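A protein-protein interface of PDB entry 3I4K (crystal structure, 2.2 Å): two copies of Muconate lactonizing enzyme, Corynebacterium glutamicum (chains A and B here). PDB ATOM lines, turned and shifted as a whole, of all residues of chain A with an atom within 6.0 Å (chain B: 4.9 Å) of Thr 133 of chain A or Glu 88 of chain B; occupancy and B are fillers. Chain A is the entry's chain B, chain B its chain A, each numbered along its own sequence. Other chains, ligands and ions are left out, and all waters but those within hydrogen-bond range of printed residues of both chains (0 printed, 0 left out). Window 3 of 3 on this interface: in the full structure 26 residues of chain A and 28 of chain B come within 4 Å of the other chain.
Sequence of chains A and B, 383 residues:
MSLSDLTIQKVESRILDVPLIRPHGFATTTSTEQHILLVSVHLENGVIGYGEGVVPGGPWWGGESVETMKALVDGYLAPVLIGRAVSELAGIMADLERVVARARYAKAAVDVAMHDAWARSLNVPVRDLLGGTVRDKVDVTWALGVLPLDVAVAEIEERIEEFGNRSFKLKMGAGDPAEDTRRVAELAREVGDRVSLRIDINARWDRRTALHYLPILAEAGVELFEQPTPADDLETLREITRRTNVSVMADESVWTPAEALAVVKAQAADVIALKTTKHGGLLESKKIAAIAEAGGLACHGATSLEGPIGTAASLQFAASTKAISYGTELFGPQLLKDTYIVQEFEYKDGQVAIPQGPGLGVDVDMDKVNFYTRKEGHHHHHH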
ATOM      1  N   ARG A 127      24.337  14.932  21.615  1.00  0.00           N
ATOM      2  CA  ARG A 127      24.743  14.650  20.243  1.00  0.00           C
ATOM      3  C   ARG A 127      24.562  15.868  19.335  1.00  0.00           C
ATOM      4  O   ARG A 127      25.284  16.034  18.350  1.00  0.00           O
ATOM      5  CB  ARG A 127      23.951  13.465  19.689  1.00  0.00           C
ATOM      6  CG  ARG A 127      22.452  13.640  19.775  1.00  0.00           C
ATOM      7  CD  ARG A 127      21.734  12.470  19.132  1.00  0.00           C
ATOM      8  NE  ARG A 127      20.288  12.675  19.100  1.00  0.00           N
ATOM      9  CZ  ARG A 127      19.484  12.528  20.148  1.00  0.00           C
ATOM     10  NH1 ARG A 127      19.977  12.164  21.326  1.00  0.00           N
ATOM     11  NH2 ARG A 127      18.184  12.757  20.019  1.00  0.00           N
ATOM     12  N   ASP A 128      23.606  16.726  19.678  1.00  0.00           N
ATOM     13  CA  ASP A 128      23.331  17.922  18.893  1.00  0.00           C
ATOM     14  C   ASP A 128      24.436  18.970  18.984  1.00  0.00           C
ATOM     15  O   ASP A 128      24.410  19.973  18.279  1.00  0.00           O
ATOM     16  CB  ASP A 128      21.982  18.513  19.306  1.00  0.00           C
ATOM     17  CG  ASP A 128      20.811  17.813  18.632  1.00  0.00           C
ATOM     18  OD1 ASP A 128      20.949  16.624  18.251  1.00  0.00           O
ATOM     19  OD2 ASP A 128      19.750  18.450  18.486  1.00  0.00           O
ATOM     20  N   GLY A 131      27.309  17.426  15.932  1.00  0.00           N
ATOM     21  CA  GLY A 131      26.952  17.111  14.559  1.00  0.00           C
ATOM     22  C   GLY A 131      25.578  16.532  14.278  1.00  0.00           C
ATOM     23  O   GLY A 131      25.197  16.396  13.116  1.00  0.00           O
ATOM     24  N   GLY A 132      24.831  16.173  15.315  1.00  0.00           N
ATOM     25  CA  GLY A 132      23.510  15.624  15.080  1.00  0.00           C
ATOM     26  C   GLY A 132      23.463  14.121  15.196  1.00  0.00           C
ATOM     27  O   GLY A 132      24.290  13.524  15.883  1.00  0.00           O
ATOM     28  N   THR A 133      22.509  13.489  14.523  1.00  0.00           N
ATOM     29  CA  THR A 133      22.414  12.044  14.622  1.00  0.00           C
ATOM     30  C   THR A 133      22.559  11.297  13.298  1.00  0.00           C
ATOM     31  O   THR A 133      22.045  11.714  12.259  1.00  0.00           O
ATOM     32  CB  THR A 133      21.087  11.618  15.300  1.00  0.00           C
ATOM     33  OG1 THR A 133      20.095  11.357  14.303  1.00  0.00           O
ATOM     34  CG2 THR A 133      20.582  12.727  16.213  1.00  0.00           C
ATOM     35  N   VAL A 134      23.277  10.185  13.361  1.00  0.00           N
ATOM     36  CA  VAL A 134      23.513   9.339  12.203  1.00  0.00           C
ATOM     37  C   VAL A 134      22.767   8.036  12.417  1.00  0.00           C
ATOM     38  O   VAL A 134      22.363   7.373  11.463  1.00  0.00           O
ATOM     39  CB  VAL A 134      25.023   9.024  12.045  1.00  0.00           C
ATOM     40  CG1 VAL A 134      25.231   7.997  10.935  1.00  0.00           C
ATOM     41  CG2 VAL A 134      25.795  10.304  11.740  1.00  0.00           C
ATOM     42  N   ARG A 135      22.592   7.681  13.687  1.00  0.00           N
ATOM     43  CA  ARG A 135      21.912   6.450  14.071  1.00  0.00           C
ATOM     44  C   ARG A 135      21.245   6.656  15.439  1.00  0.00           C
ATOM     45  O   ARG A 135      21.574   7.599  16.151  1.00  0.00           O
ATOM     46  CB  ARG A 135      22.941   5.320  14.150  1.00  0.00           C
ATOM     47  CG  ARG A 135      24.091   5.623  15.112  1.00  0.00           C
ATOM     48  CD  ARG A 135      25.103   4.487  15.228  1.00  0.00           C
ATOM     49  NE  ARG A 135      26.312   4.705  14.431  1.00  0.00           N
ATOM     50  CZ  ARG A 135      26.463   4.302  13.175  1.00  0.00           C
ATOM     51  NH1 ARG A 135      25.477   3.655  12.565  1.00  0.00           N
ATOM     52  NH2 ARG A 135      27.599   4.539  12.530  1.00  0.00           N
ATOM     53  N   ASP A 136      20.310   5.781  15.804  1.00  0.00           N
ATOM     54  CA  ASP A 136      19.623   5.896  17.096  1.00  0.00           C
ATOM     55  C   ASP A 136      19.735   4.622  17.934  1.00  0.00           C
ATOM     56  O   ASP A 136      19.145   4.513  19.011  1.00  0.00           O
ATOM     57  CB  ASP A 136      18.149   6.244  16.893  1.00  0.00           C
ATOM     58  CG  ASP A 136      17.430   5.233  16.032  1.00  0.00           C
ATOM     59  OD1 ASP A 136      17.523   4.023  16.329  1.00  0.00           O
ATOM     60  OD2 ASP A 136      16.767   5.649  15.060  1.00  0.00           O
ATOM     61  N   ALA A 319      26.000   8.080  18.379  1.00  0.00           N
ATOM     62  CA  ALA A 319      24.848   8.518  17.600  1.00  0.00           C
ATOM     63  C   ALA A 319      25.247   9.545  16.551  1.00  0.00           C
ATOM     64  O   ALA A 319      24.662   9.604  15.478  1.00  0.00           O
ATOM     65  CB  ALA A 319      23.790   9.124  18.525  1.00  0.00           C
ATOM     66  N   SER A 320      26.257  10.344  16.866  1.00  0.00           N
ATOM     67  CA  SER A 320      26.703  11.407  15.977  1.00  0.00           C
ATOM     68  C   SER A 320      27.972  11.133  15.163  1.00  0.00           C
ATOM     69  O   SER A 320      28.385  11.976  14.367  1.00  0.00           O
ATOM     70  CB  SER A 320      26.923  12.671  16.808  1.00  0.00           C
ATOM     71  OG  SER A 320      27.896  12.437  17.818  1.00  0.00           O
ATOM     72  N   ARG B  84      13.817  15.739   5.837  1.00  0.00           N
ATOM     73  CA  ARG B  84      14.591  15.304   7.000  1.00  0.00           C
ATOM     74  C   ARG B  84      14.880  16.466   7.934  1.00  0.00           C
ATOM     75  O   ARG B  84      14.935  17.613   7.498  1.00  0.00           O
ATOM     76  CB  ARG B  84      15.909  14.666   6.554  1.00  0.00           C
ATOM     77  CG  ARG B  84      15.722  13.428   5.698  1.00  0.00           C
ATOM     78  CD  ARG B  84      17.045  12.854   5.228  1.00  0.00           C
ATOM     79  NE  ARG B  84      17.838  12.312   6.329  1.00  0.00           N
ATOM     80  CZ  ARG B  84      19.001  11.691   6.164  1.00  0.00           C
ATOM     81  NH1 ARG B  84      19.501  11.538   4.941  1.00  0.00           N
ATOM     82  NH2 ARG B  84      19.664  11.222   7.214  1.00  0.00           N
ATOM     83  N   ALA B  85      15.055  16.169   9.218  1.00  0.00           N
ATOM     84  CA  ALA B  85      15.346  17.206  10.205  1.00  0.00           C
ATOM     85  C   ALA B  85      16.780  17.694  10.019  1.00  0.00           C
ATOM     86  O   ALA B  85      17.682  16.900   9.758  1.00  0.00           O
ATOM     87  CB  ALA B  85      15.156  16.655  11.619  1.00  0.00           C
ATOM     88  N   VAL B  86      16.990  18.998  10.155  1.00  0.00           N
ATOM     89  CA  VAL B  86      18.319  19.572   9.995  1.00  0.00           C
ATOM     90  C   VAL B  86      19.217  19.077  11.129  1.00  0.00           C
ATOM     91  O   VAL B  86      20.444  19.173  11.052  1.00  0.00           O
ATOM     92  CB  VAL B  86      18.263  21.122  10.005  1.00  0.00           C
ATOM     93  CG1 VAL B  86      18.047  21.625  11.413  1.00  0.00           C
ATOM     94  CG2 VAL B  86      19.546  21.706   9.418  1.00  0.00           C
ATOM     95  N   SER B  87      18.593  18.543  12.177  1.00  0.00           N
ATOM     96  CA  SER B  87      19.324  18.028  13.324  1.00  0.00           C
ATOM     97  C   SER B  87      19.925  16.656  13.008  1.00  0.00           C
ATOM     98  O   SER B  87      20.492  16.002  13.877  1.00  0.00           O
ATOM     99  CB  SER B  87      18.402  17.935  14.551  1.00  0.00           C
ATOM    100  OG  SER B  87      17.374  16.976  14.365  1.00  0.00           O
ATOM    101  N   GLU B  88      19.784  16.226  11.758  1.00  0.00           N
ATOM    102  CA  GLU B  88      20.345  14.955  11.295  1.00  0.00           C
ATOM    103  C   GLU B  88      21.585  15.286  10.469  1.00  0.00           C
ATOM    104  O   GLU B  88      22.096  14.448   9.731  1.00  0.00           O
ATOM    105  CB  GLU B  88      19.357  14.213  10.397  1.00  0.00           C
ATOM    106  CG  GLU B  88      18.219  13.532  11.115  1.00  0.00           C
ATOM    107  CD  GLU B  88      17.258  12.876  10.150  1.00  0.00           C
ATOM    108  OE1 GLU B  88      17.684  11.986   9.386  1.00  0.00           O
ATOM    109  OE2 GLU B  88      16.070  13.258  10.154  1.00  0.00           O
ATOM    110  N   LEU B  89      22.037  16.524  10.596  1.00  0.00           N
ATOM    111  CA  LEU B  89      23.189  17.041   9.876  1.00  0.00           C
ATOM    112  C   LEU B  89      24.243  15.974   9.542  1.00  0.00           C
ATOM    113  O   LEU B  89      24.400  15.596   8.373  1.00  0.00           O
ATOM    114  CB  LEU B  89      23.802  18.190  10.693  1.00  0.00           C
ATOM    115  CG  LEU B  89      24.961  19.068  10.200  1.00  0.00           C
ATOM    116  CD1 LEU B  89      25.385  18.722   8.782  1.00  0.00           C
ATOM    117  CD2 LEU B  89      24.528  20.510  10.309  1.00  0.00           C
ATOM    118  N   ALA B  90      24.943  15.475  10.556  1.00  0.00           N
ATOM    119  CA  ALA B  90      25.980  14.467  10.329  1.00  0.00           C
ATOM    120  C   ALA B  90      25.523  13.273   9.492  1.00  0.00           C
ATOM    121  O   ALA B  90      26.260  12.807   8.623  1.00  0.00           O
ATOM    122  CB  ALA B  90      26.542  13.983  11.659  1.00  0.00           C
ATOM    123  N   GLY B  91      24.317  12.776   9.745  1.00  0.00           N
ATOM    124  CA  GLY B  91      23.823  11.637   8.989  1.00  0.00           C
ATOM    125  C   GLY B  91      23.551  11.969   7.531  1.00  0.00           C
ATOM    126  O   GLY B  91      23.776  11.151   6.636  1.00  0.00           O
ATOM    127  N   ILE B  92      23.062  13.180   7.290  1.00  0.00           N
ATOM    128  CA  ILE B  92      22.760  13.613   5.936  1.00  0.00           C
ATOM    129  C   ILE B  92      24.060  13.749   5.151  1.00  0.00           C
ATOM    130  O   ILE B  92      24.156  13.275   4.017  1.00  0.00           O
ATOM    131  CB  ILE B  92      21.988  14.949   5.959  1.00  0.00           C
ATOM    132  CG1 ILE B  92      20.617  14.727   6.616  1.00  0.00           C
ATOM    133  CG2 ILE B  92      21.833  15.494   4.551  1.00  0.00           C
ATOM    134  CD1 ILE B  92      19.831  15.988   6.847  1.00  0.00           C
ATOM    135  N   MET B 114      23.020  24.015   6.308  1.00  0.00           N
ATOM    136  CA  MET B 114      22.379  23.230   7.353  1.00  0.00           C
ATOM    137  C   MET B 114      22.790  23.684   8.748  1.00  0.00           C
ATOM    138  O   MET B 114      21.968  23.718   9.667  1.00  0.00           O
ATOM    139  CB  MET B 114      22.683  21.747   7.165  1.00  0.00           C
ATOM    140  CG  MET B 114      21.925  21.144   6.003  1.00  0.00           C
ATOM    141  SD  MET B 114      21.836  19.228   6.102  1.00  0.00           S
ATOM    142  CE  MET B 114      21.135  19.054   7.891  1.00  0.00           C
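Among the printed residues, pairs that only touch across the chains: Gly 131 of chain A with Leu 89 of chain B (3.3 Å), Gly 132 of chain A with Ser 87 of chain B (3.3 Å), Thr 133 of chain A with Glu 88 of chain B (3.7 Å), Thr 133 of chain A with Gly 91 of chain B (3.6 Å), Val 134 of chain A with Ala 90 of chain B (3.7 Å), Val 134 of chain A with Gly 91 of chain B (3.5 Å) and Ser 320 of chain A with Ala 90 of chain B (3.8 Å).
Thr 133 of chain A touches three residues of chain B. Glu 88 of chain B touches just one residue of chain A: Thr 133. Of the printed residues of chain A, Leu 89 of chain B touches Gly 131. Printed residues of chain A within 4 Å of Gly 91 of chain B: Thr 133 (3.6 Å) and Val 134 (3.5 Å). Of the printed residues of chain A, Ser 87 of chain B touches Gly 132 and Thr 133. Of the printed residues of chain A, Ala 90 of chain B touches Gly 131, Val 134 and Ser 320. Of the printed residues of chain B, Val 134 of chain A touches Ala 90 (3.7 Å) and Gly 91 (3.5 Å). The nearest residue of chain A that does not touch Glu 88 of chain B is Gly 131 of chain A (4.6 Å).
No position is printed for both chains. Of the 9 pairs that touch across the chains among the printed residues, none has its exchanged pair printed and touching as well.
Of the 10 printed residues of chain B, 5 touch a printed residue of chain A. Of the 10 printed residues of chain A, 5 touch a printed residue of chain B.
The backbone NH of Thr 133 of chain A lies within hydrogen-bond range of the backbone carbonyl oxygen of Ser 87 of chain B (3.3 Å). The backbone NH (N) of Ala 90 of chain B lies within hydrogen-bond range of the backbone carbonyl oxygen (O) of Gly 131 of chain A, at 2.7 Å.
The guanidinium group (NH2) of Arg 84 of chain B is in salt-bridge range of the side-chain carboxylate (OE1) of Glu 88 of chain B, at 3.0 Å. The backbone NH (N) of Ala 85 of chain B sits at hydrogen-bond distance from the side-chain carboxylate (OE2) of Glu 88 of chain B, 3.2 Å away. The backbone carbonyl oxygen (O) of Arg 127 of chain A is in hydrogen-bond range of the backbone NH (N) of Gly 132 of chain A, at 3.1 Å. The backbone NH of Val 134 of chain A sits at hydrogen-bond distance from the backbone carbonyl oxygen of Ala 319 of chain A (2.6 Å).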
